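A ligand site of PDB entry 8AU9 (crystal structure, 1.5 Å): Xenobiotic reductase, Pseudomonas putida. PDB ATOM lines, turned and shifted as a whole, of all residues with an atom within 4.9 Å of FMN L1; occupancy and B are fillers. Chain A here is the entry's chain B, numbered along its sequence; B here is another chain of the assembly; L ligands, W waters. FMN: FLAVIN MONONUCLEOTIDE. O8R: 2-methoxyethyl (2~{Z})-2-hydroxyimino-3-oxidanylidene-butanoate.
NE2 of Gln 99 lies within hydrogen-bond range of OE2 of Glu 176 (2.8 Å).
The backbone NH of Ala 57 sits close to the side-chain amide oxygen of Gln 99, 3.4 Å away.
Water W2 bridges O2P of FMN L1 (2.8 Å) and N of Arg 326 (3.4 Å).
A ring nitrogen (ND1) of His 181 lies close to an oxygen (O2) of FMN L1, 3.4 Å away.
N of Gly 325 lies within hydrogen-bond range of O2P of FMN L1, at 2.8 Å.
O2' of FMN L1 lies within hydrogen-bond range of NH1 of Arg 231.
OE1 of Gln 99 is in hydrogen-bond range of N3 of FMN L1 (2.8 Å).
N of Ala 57 sits at hydrogen-bond distance from O4 of FMN L1, at 3.2 Å.
An oxygen (O5') of FMN L1 lies within hydrogen-bond range of the backbone NH (N) of Trp 302 (3.1 Å).
The backbone carbonyl oxygen (O) of Pro 23 lies close to an oxygen (O2') of FMN L1 (2.9 Å).
N of Arg 326 lies within hydrogen-bond range of O1P of FMN L1 (2.8 Å).
A ring nitrogen (ND1) of His 181 lies within hydrogen-bond range of an oxygen (O4) of O8R L2 (2.6 Å).
The guanidinium group (NE) of Arg 326 lies within salt-bridge range of an oxygen (O1P) of FMN L1 (2.7 Å).
The side-chain sulfur (SG) of Cys 25 is in hydrogen-bond range of an oxygen (O4) of FMN L1, 3.2 Å away.
An oxygen (O4) of O8R L2 lies within hydrogen-bond range of a ring nitrogen (NE2) of His 178 (2.8 Å).
The backbone NH (N) of Cys 25 lies within hydrogen-bond range of a nitrogen (N5) of FMN L1 (2.8 Å).
An oxygen (O2) of FMN L1 sits at hydrogen-bond distance from a ring nitrogen (NE2) of His 178 (3.3 Å).
N of Gly 303 sits at hydrogen-bond distance from O3P of FMN L1 (3.1 Å).
Residues that only touch FMN L1: Pro 22 (3.4 Å), Met 24 (3.1 Å), Ala 301 (3.5 Å), Ser 323 (3.9 Å), Val 324 (3.7 Å) and Trp 358 of chain B (3.1 Å).
Hydrophobic or aromatic side chains within 4 Å of FMN L1: Pro 22, Pro 23, Met 24, Ala 57, His 178, His 181, Ala 301, Trp 302 and Trp 358 of chain B.
Of the 23 residues printed, 17 come within 4 Å of FMN L1.
O4 of O8R L2 lies close to N3 of FMN L1 (3.1 Å).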
ATOM      1  N   PRO A  22      -5.468  -8.503  15.477  1.00  0.00           N
ATOM      2  CA  PRO A  22      -6.422  -8.458  16.580  1.00  0.00           C
ATOM      3  C   PRO A  22      -7.590  -9.385  16.311  1.00  0.00           C
ATOM      4  O   PRO A  22      -7.792  -9.825  15.163  1.00  0.00           O
ATOM      5  CB  PRO A  22      -6.877  -6.987  16.582  1.00  0.00           C
ATOM      6  CG  PRO A  22      -6.782  -6.598  15.124  1.00  0.00           C
ATOM      7  CD  PRO A  22      -5.575  -7.331  14.580  1.00  0.00           C
ATOM      8  N   PRO A  23      -8.383  -9.697  17.320  1.00  0.00           N
ATOM      9  CA  PRO A  23      -9.535 -10.588  17.113  1.00  0.00           C
ATOM     10  C   PRO A  23     -10.500  -9.991  16.104  1.00  0.00           C
ATOM     11  O   PRO A  23     -10.838  -8.811  16.181  1.00  0.00           O
ATOM     12  CB  PRO A  23     -10.170 -10.684  18.503  1.00  0.00           C
ATOM     13  CG  PRO A  23      -9.651  -9.438  19.253  1.00  0.00           C
ATOM     14  CD  PRO A  23      -8.267  -9.250  18.729  1.00  0.00           C
ATOM     15  N   MET A  24     -10.907 -10.815  15.140  1.00  0.00           N
ATOM     16  CA  MET A  24     -11.861 -10.380  14.107  1.00  0.00           C
ATOM     17  C   MET A  24     -12.896 -11.464  13.872  1.00  0.00           C
ATOM     18  O   MET A  24     -12.603 -12.473  13.221  1.00  0.00           O
ATOM     19  CB  MET A  24     -11.164  -9.944  12.821  1.00  0.00           C
ATOM     20  CG  MET A  24     -10.467  -8.592  12.951  1.00  0.00           C
ATOM     21  SD  MET A  24      -9.663  -8.126  11.402  1.00  0.00           S
ATOM     22  CE  MET A  24      -8.408  -9.406  11.306  1.00  0.00           C
ATOM     23  N   CYS A  25     -14.107 -11.266  14.401  1.00  0.00           N
ATOM     24  CA  CYS A  25     -15.216 -12.191  14.192  1.00  0.00           C
ATOM     25  C   CYS A  25     -15.420 -12.472  12.714  1.00  0.00           C
ATOM     26  O   CYS A  25     -15.412 -11.561  11.883  1.00  0.00           O
ATOM     27  CB  CYS A  25     -16.506 -11.577  14.732  1.00  0.00           C
ATOM     28  SG  CYS A  25     -16.739 -11.751  16.515  1.00  0.00           S
ATOM     29  N   GLU A  56     -10.652 -14.497  16.985  1.00  0.00           N
ATOM     30  CA  GLU A  56     -11.868 -13.718  17.180  1.00  0.00           C
ATOM     31  C   GLU A  56     -12.573 -13.980  18.497  1.00  0.00           C
ATOM     32  O   GLU A  56     -12.400 -15.045  19.099  1.00  0.00           O
ATOM     33  CB  GLU A  56     -12.858 -14.075  16.076  1.00  0.00           C
ATOM     34  CG  GLU A  56     -13.275 -15.553  16.073  1.00  0.00           C
ATOM     35  CD  GLU A  56     -13.942 -15.948  14.753  1.00  0.00           C
ATOM     36  OE1 GLU A  56     -15.150 -15.731  14.608  1.00  0.00           O
ATOM     37  OE2 GLU A  56     -13.220 -16.442  13.843  1.00  0.00           O
ATOM     38  N   ALA A  57     -13.381 -13.011  18.941  1.00  0.00           N
ATOM     39  CA  ALA A  57     -14.248 -13.134  20.104  1.00  0.00           C
ATOM     40  C   ALA A  57     -14.953 -14.485  20.110  1.00  0.00           C
ATOM     41  O   ALA A  57     -15.758 -14.793  19.227  1.00  0.00           O
ATOM     42  CB  ALA A  57     -15.282 -12.014  20.129  1.00  0.00           C
ATOM     43  N   GLN A  99      -9.350 -14.465  22.081  1.00  0.00           N
ATOM     44  CA  GLN A  99     -10.161 -13.551  22.865  1.00  0.00           C
ATOM     45  C   GLN A  99     -11.415 -14.287  23.313  1.00  0.00           C
ATOM     46  O   GLN A  99     -12.170 -14.790  22.477  1.00  0.00           O
ATOM     47  CB  GLN A  99     -10.551 -12.338  22.024  1.00  0.00           C
ATOM     48  CG  GLN A  99     -11.281 -11.266  22.832  1.00  0.00           C
ATOM     49  CD  GLN A  99     -11.846 -10.179  21.948  1.00  0.00           C
ATOM     50  OE1 GLN A  99     -12.641 -10.454  21.044  1.00  0.00           O
ATOM     51  NE2 GLN A  99     -11.453  -8.930  22.209  1.00  0.00           N
ATOM     52  N   GLU A 176      -6.884 -13.182  25.791  1.00  0.00           N
ATOM     53  CA  GLU A 176      -7.380 -11.809  25.896  1.00  0.00           C
ATOM     54  C   GLU A 176      -8.817 -11.848  26.397  1.00  0.00           C
ATOM     55  O   GLU A 176      -9.690 -12.444  25.749  1.00  0.00           O
ATOM     56  CB  GLU A 176      -7.312 -11.102  24.530  1.00  0.00           C
ATOM     57  CG  GLU A 176      -7.717  -9.629  24.582  1.00  0.00           C
ATOM     58  CD  GLU A 176      -7.672  -8.972  23.211  1.00  0.00           C
ATOM     59  OE1 GLU A 176      -6.570  -8.804  22.647  1.00  0.00           O
ATOM     60  OE2 GLU A 176      -8.749  -8.614  22.696  1.00  0.00           O
ATOM     61  N   HIS A 178     -12.297 -10.175  26.807  1.00  0.00           N
ATOM     62  CA  HIS A 178     -12.973  -9.132  26.033  1.00  0.00           C
ATOM     63  C   HIS A 178     -13.791  -8.245  26.972  1.00  0.00           C
ATOM     64  O   HIS A 178     -14.969  -8.497  27.229  1.00  0.00           O
ATOM     65  CB  HIS A 178     -13.862  -9.729  24.947  1.00  0.00           C
ATOM     66  CG  HIS A 178     -14.234  -8.735  23.900  1.00  0.00           C
ATOM     67  ND1 HIS A 178     -14.015  -7.385  24.050  1.00  0.00           N
ATOM     68  CD2 HIS A 178     -14.793  -8.894  22.673  1.00  0.00           C
ATOM     69  CE1 HIS A 178     -14.427  -6.749  22.966  1.00  0.00           C
ATOM     70  NE2 HIS A 178     -14.902  -7.651  22.110  1.00  0.00           N
ATOM     71  N   HIS A 181     -15.844  -2.639  23.942  1.00  0.00           N
ATOM     72  CA  HIS A 181     -16.745  -2.578  22.802  1.00  0.00           C
ATOM     73  C   HIS A 181     -18.222  -2.720  23.178  1.00  0.00           C
ATOM     74  O   HIS A 181     -19.038  -3.102  22.328  1.00  0.00           O
ATOM     75  CB  HIS A 181     -16.317  -3.568  21.704  1.00  0.00           C
ATOM     76  CG  HIS A 181     -14.929  -3.320  21.203  1.00  0.00           C
ATOM     77  ND1 HIS A 181     -14.253  -4.207  20.382  1.00  0.00           N
ATOM     78  CD2 HIS A 181     -14.080  -2.281  21.403  1.00  0.00           C
ATOM     79  CE1 HIS A 181     -13.053  -3.718  20.104  1.00  0.00           C
ATOM     80  NE2 HIS A 181     -12.930  -2.554  20.721  1.00  0.00           N
ATOM     81  N   ARG A 231      -8.788  -6.661  26.556  1.00  0.00           N
ATOM     82  CA  ARG A 231      -9.132  -5.506  25.742  1.00  0.00           C
ATOM     83  C   ARG A 231     -10.149  -4.672  26.503  1.00  0.00           C
ATOM     84  O   ARG A 231     -11.091  -5.215  27.084  1.00  0.00           O
ATOM     85  CB  ARG A 231      -9.691  -5.934  24.378  1.00  0.00           C
ATOM     86  CG  ARG A 231      -9.809  -4.786  23.395  1.00  0.00           C
ATOM     87  CD  ARG A 231     -10.014  -5.259  21.964  1.00  0.00           C
ATOM     88  NE  ARG A 231      -9.259  -4.401  21.040  1.00  0.00           N
ATOM     89  CZ  ARG A 231      -9.278  -4.536  19.712  1.00  0.00           C
ATOM     90  NH1 ARG A 231     -10.024  -5.458  19.139  1.00  0.00           N
ATOM     91  NH2 ARG A 231      -8.544  -3.715  18.967  1.00  0.00           N
ATOM     92  N   ALA A 301      -5.415  -0.280  17.975  1.00  0.00           N
ATOM     93  CA  ALA A 301      -5.850  -0.548  16.612  1.00  0.00           C
ATOM     94  C   ALA A 301      -6.610   0.672  16.121  1.00  0.00           C
ATOM     95  O   ALA A 301      -6.458   1.772  16.662  1.00  0.00           O
ATOM     96  CB  ALA A 301      -6.680  -1.841  16.551  1.00  0.00           C
ATOM     97  N   TRP A 302      -7.436   0.482  15.077  1.00  0.00           N
ATOM     98  CA  TRP A 302      -8.330   1.496  14.536  1.00  0.00           C
ATOM     99  C   TRP A 302      -7.582   2.560  13.749  1.00  0.00           C
ATOM    100  O   TRP A 302      -7.760   3.758  13.995  1.00  0.00           O
ATOM    101  CB  TRP A 302      -9.204   2.158  15.607  1.00  0.00           C
ATOM    102  CG  TRP A 302      -9.925   1.182  16.494  1.00  0.00           C
ATOM    103  CD1 TRP A 302      -9.564   0.789  17.755  1.00  0.00           C
ATOM    104  CD2 TRP A 302     -11.129   0.465  16.171  1.00  0.00           C
ATOM    105  NE1 TRP A 302     -10.474  -0.128  18.241  1.00  0.00           N
ATOM    106  CE2 TRP A 302     -11.445  -0.336  17.289  1.00  0.00           C
ATOM    107  CE3 TRP A 302     -11.970   0.442  15.056  1.00  0.00           C
ATOM    108  CZ2 TRP A 302     -12.566  -1.174  17.315  1.00  0.00           C
ATOM    109  CZ3 TRP A 302     -13.081  -0.399  15.083  1.00  0.00           C
ATOM    110  CH2 TRP A 302     -13.372  -1.181  16.215  1.00  0.00           C
ATOM    111  N   GLY A 303      -6.762   2.154  12.789  1.00  0.00           N
ATOM    112  CA  GLY A 303      -6.138   3.115  11.910  1.00  0.00           C
ATOM    113  C   GLY A 303      -4.627   3.113  11.900  1.00  0.00           C
ATOM    114  O   GLY A 303      -4.016   4.084  11.457  1.00  0.00           O
ATOM    115  N   PHE A 304      -4.004   2.034  12.372  1.00  0.00           N
ATOM    116  CA  PHE A 304      -2.557   1.891  12.303  1.00  0.00           C
ATOM    117  C   PHE A 304      -2.106   1.087  11.095  1.00  0.00           C
ATOM    118  O   PHE A 304      -0.913   0.792  10.972  1.00  0.00           O
ATOM    119  CB  PHE A 304      -2.002   1.254  13.583  1.00  0.00           C
ATOM    120  CG  PHE A 304      -2.139   2.115  14.808  1.00  0.00           C
ATOM    121  CD1 PHE A 304      -1.241   3.153  15.050  1.00  0.00           C
ATOM    122  CD2 PHE A 304      -3.128   1.867  15.740  1.00  0.00           C
ATOM    123  CE1 PHE A 304      -1.352   3.938  16.193  1.00  0.00           C
ATOM    124  CE2 PHE A 304      -3.249   2.656  16.883  1.00  0.00           C
ATOM    125  CZ  PHE A 304      -2.354   3.678  17.108  1.00  0.00           C
ATOM    126  N   GLY A 305      -3.028   0.725  10.210  1.00  0.00           N
ATOM    127  CA  GLY A 305      -2.752  -0.241   9.160  1.00  0.00           C
ATOM    128  C   GLY A 305      -1.986   0.241   7.942  1.00  0.00           C
ATOM    129  O   GLY A 305      -2.317  -0.136   6.809  1.00  0.00           O
ATOM    130  N   SER A 323      -1.659  -3.539  16.401  1.00  0.00           N
ATOM    131  CA  SER A 323      -2.694  -4.438  15.921  1.00  0.00           C
ATOM    132  C   SER A 323      -3.190  -3.948  14.570  1.00  0.00           C
ATOM    133  O   SER A 323      -3.583  -2.789  14.425  1.00  0.00           O
ATOM    134  CB  SER A 323      -3.837  -4.544  16.928  1.00  0.00           C
ATOM    135  OG  SER A 323      -3.395  -5.198  18.121  1.00  0.00           O
ATOM    136  N   VAL A 324      -3.133  -4.826  13.571  1.00  0.00           N
ATOM    137  CA  VAL A 324      -3.495  -4.501  12.193  1.00  0.00           C
ATOM    138  C   VAL A 324      -4.567  -5.491  11.774  1.00  0.00           C
ATOM    139  O   VAL A 324      -4.272  -6.674  11.542  1.00  0.00           O
ATOM    140  CB  VAL A 324      -2.278  -4.534  11.259  1.00  0.00           C
ATOM    141  CG1 VAL A 324      -2.687  -4.204   9.819  1.00  0.00           C
ATOM    142  CG2 VAL A 324      -1.220  -3.543  11.741  1.00  0.00           C
ATOM    143  N   GLY A 325      -5.805  -5.023  11.678  1.00  0.00           N
ATOM    144  CA  GLY A 325      -6.940  -5.894  11.443  1.00  0.00           C
ATOM    145  C   GLY A 325      -7.393  -5.935   9.991  1.00  0.00           C
ATOM    146  O   GLY A 325      -7.072  -6.888   9.270  1.00  0.00           O
ATOM    147  N   ARG A 326      -8.123  -4.902   9.556  1.00  0.00           N
ATOM    148  CA  ARG A 326      -8.711  -4.958   8.215  1.00  0.00           C
ATOM    149  C   ARG A 326      -7.679  -5.143   7.111  1.00  0.00           C
ATOM    150  O   ARG A 326      -7.981  -5.777   6.087  1.00  0.00           O
ATOM    151  CB  ARG A 326      -9.574  -3.719   7.972  1.00  0.00           C
ATOM    152  CG  ARG A 326     -10.922  -3.802   8.693  1.00  0.00           C
ATOM    153  CD  ARG A 326     -11.598  -2.447   8.786  1.00  0.00           C
ATOM    154  NE  ARG A 326     -10.849  -1.525   9.641  1.00  0.00           N
ATOM    155  CZ  ARG A 326     -11.215  -0.267   9.841  1.00  0.00           C
ATOM    156  NH1 ARG A 326     -12.296   0.219   9.245  1.00  0.00           N
ATOM    157  NH2 ARG A 326     -10.487   0.522  10.632  1.00  0.00           N
ATOM    158  N   LEU A 329      -7.414  -8.689   6.395  1.00  0.00           N
ATOM    159  CA  LEU A 329      -8.506  -9.246   5.604  1.00  0.00           C
ATOM    160  C   LEU A 329      -8.297  -8.938   4.126  1.00  0.00           C
ATOM    161  O   LEU A 329      -8.576  -9.766   3.265  1.00  0.00           O
ATOM    162  CB  LEU A 329      -9.842  -8.667   6.061  1.00  0.00           C
ATOM    163  CG  LEU A 329     -10.184  -8.770   7.553  1.00  0.00           C
ATOM    164  CD1 LEU A 329     -11.579  -8.222   7.822  1.00  0.00           C
ATOM    165  CD2 LEU A 329     -10.050 -10.207   8.039  1.00  0.00           C
ATOM    166  N   PRO B 354     -17.276 -12.493   4.772  1.00  0.00           N
ATOM    167  CA  PRO B 354     -16.617 -12.101   6.040  1.00  0.00           C
ATOM    168  C   PRO B 354     -15.487 -11.106   5.861  1.00  0.00           C
ATOM    169  O   PRO B 354     -15.060 -10.478   6.843  1.00  0.00           O
ATOM    170  CB  PRO B 354     -16.107 -13.431   6.611  1.00  0.00           C
ATOM    171  CG  PRO B 354     -16.973 -14.474   5.963  1.00  0.00           C
ATOM    172  CD  PRO B 354     -17.209 -13.951   4.565  1.00  0.00           C
ATOM    173  N   TRP B 358     -16.553  -5.698   5.223  1.00  0.00           N
ATOM    174  CA  TRP B 358     -15.778  -4.734   5.991  1.00  0.00           C
ATOM    175  C   TRP B 358     -14.865  -3.893   5.121  1.00  0.00           C
ATOM    176  O   TRP B 358     -14.528  -2.760   5.481  1.00  0.00           O
ATOM    177  CB  TRP B 358     -14.956  -5.474   7.035  1.00  0.00           C
ATOM    178  CG  TRP B 358     -15.828  -6.331   7.857  1.00  0.00           C
ATOM    179  CD1 TRP B 358     -16.052  -7.660   7.701  1.00  0.00           C
ATOM    180  CD2 TRP B 358     -16.639  -5.898   8.944  1.00  0.00           C
ATOM    181  NE1 TRP B 358     -16.968  -8.101   8.637  1.00  0.00           N
ATOM    182  CE2 TRP B 358     -17.335  -7.031   9.417  1.00  0.00           C
ATOM    183  CE3 TRP B 358     -16.852  -4.670   9.568  1.00  0.00           C
ATOM    184  CZ2 TRP B 358     -18.211  -6.973  10.494  1.00  0.00           C
ATOM    185  CZ3 TRP B 358     -17.719  -4.615  10.646  1.00  0.00           C
ATOM    186  CH2 TRP B 358     -18.396  -5.761  11.091  1.00  0.00           C
HETATM  187  N1  FMN L   1     -12.553  -6.551  18.049  1.00  0.00           N
HETATM  188  C2  FMN L   1     -12.686  -7.370  19.136  1.00  0.00           C
HETATM  189  O2  FMN L   1     -12.277  -6.985  20.224  1.00  0.00           O
HETATM  190  N3  FMN L   1     -13.245  -8.626  19.017  1.00  0.00           N
HETATM  191  C4  FMN L   1     -13.706  -9.079  17.805  1.00  0.00           C
HETATM  192  O4  FMN L   1     -14.189 -10.204  17.686  1.00  0.00           O
HETATM  193  C4A FMN L   1     -13.571  -8.254  16.705  1.00  0.00           C
HETATM  194  N5  FMN L   1     -14.026  -8.688  15.487  1.00  0.00           N
HETATM  195  C5A FMN L   1     -13.874  -7.880  14.382  1.00  0.00           C
HETATM  196  C6  FMN L   1     -14.331  -8.359  13.157  1.00  0.00           C
HETATM  197  C7  FMN L   1     -14.197  -7.589  12.021  1.00  0.00           C
HETATM  198  C7M FMN L   1     -14.671  -8.155  10.708  1.00  0.00           C
HETATM  199  C8  FMN L   1     -13.627  -6.337  12.100  1.00  0.00           C
HETATM  200  C8M FMN L   1     -13.488  -5.493  10.858  1.00  0.00           C
HETATM  201  C9  FMN L   1     -13.177  -5.844  13.331  1.00  0.00           C
HETATM  202  C9A FMN L   1     -13.294  -6.625  14.480  1.00  0.00           C
HETATM  203  N10 FMN L   1     -12.867  -6.175  15.725  1.00  0.00           N
HETATM  204  C10 FMN L   1     -12.990  -6.993  16.823  1.00  0.00           C
HETATM  205  C1' FMN L   1     -12.197  -4.850  15.852  1.00  0.00           C
HETATM  206  C2' FMN L   1     -10.744  -5.139  15.388  1.00  0.00           C
HETATM  207  O2' FMN L   1     -10.088  -6.031  16.283  1.00  0.00           O
HETATM  208  C3' FMN L   1      -9.917  -3.874  15.217  1.00  0.00           C
HETATM  209  O3' FMN L   1      -9.900  -3.176  16.437  1.00  0.00           O
HETATM  210  C4' FMN L   1     -10.510  -2.979  14.142  1.00  0.00           C
HETATM  211  O4' FMN L   1     -10.656  -3.695  12.920  1.00  0.00           O
HETATM  212  C5' FMN L   1      -9.636  -1.741  13.926  1.00  0.00           C
HETATM  213  O5' FMN L   1      -8.336  -2.056  13.483  1.00  0.00           O
HETATM  214  P   FMN L   1      -7.915  -1.860  11.941  1.00  0.00           P
HETATM  215  O1P FMN L   1      -8.885  -2.707  11.131  1.00  0.00           O
HETATM  216  O2P FMN L   1      -6.492  -2.313  11.799  1.00  0.00           O
HETATM  217  O3P FMN L   1      -8.083  -0.395  11.625  1.00  0.00           O
HETATM  218  N1  O8R L   2     -16.158  -6.849  18.526  1.00  0.00           N
HETATM  219  C4  O8R L   2     -16.028  -4.566  17.653  1.00  0.00           C
HETATM  220  C5  O8R L   2     -16.368  -2.349  18.314  1.00  0.00           C
HETATM  221  C6  O8R L   2     -17.025  -1.548  17.195  1.00  0.00           C
HETATM  222  C7  O8R L   2     -19.140  -0.809  16.481  1.00  0.00           C
HETATM  223  C1  O8R L   2     -17.952  -5.467  15.561  1.00  0.00           C
HETATM  224  C2  O8R L   2     -17.349  -6.516  16.495  1.00  0.00           C
HETATM  225  C3  O8R L   2     -16.471  -6.032  17.626  1.00  0.00           C
HETATM  226  O1  O8R L   2     -17.574  -7.686  16.363  1.00  0.00           O
HETATM  227  O2  O8R L   2     -15.021  -4.193  17.142  1.00  0.00           O
HETATM  228  O3  O8R L   2     -16.861  -3.649  18.290  1.00  0.00           O
HETATM  229  O4  O8R L   2     -15.358  -6.440  19.588  1.00  0.00           O
HETATM  230  O5  O8R L   2     -18.417  -1.706  17.282  1.00  0.00           O
HETATM  231  O   HOH W   1      -5.999   0.599   9.995  1.00  0.00           O
HETATM  232  O   HOH W   2      -5.765  -2.487   9.056  1.00  0.00           O
HETATM  233  O   HOH W   3      -4.821  -0.712  13.192  1.00  0.00           O
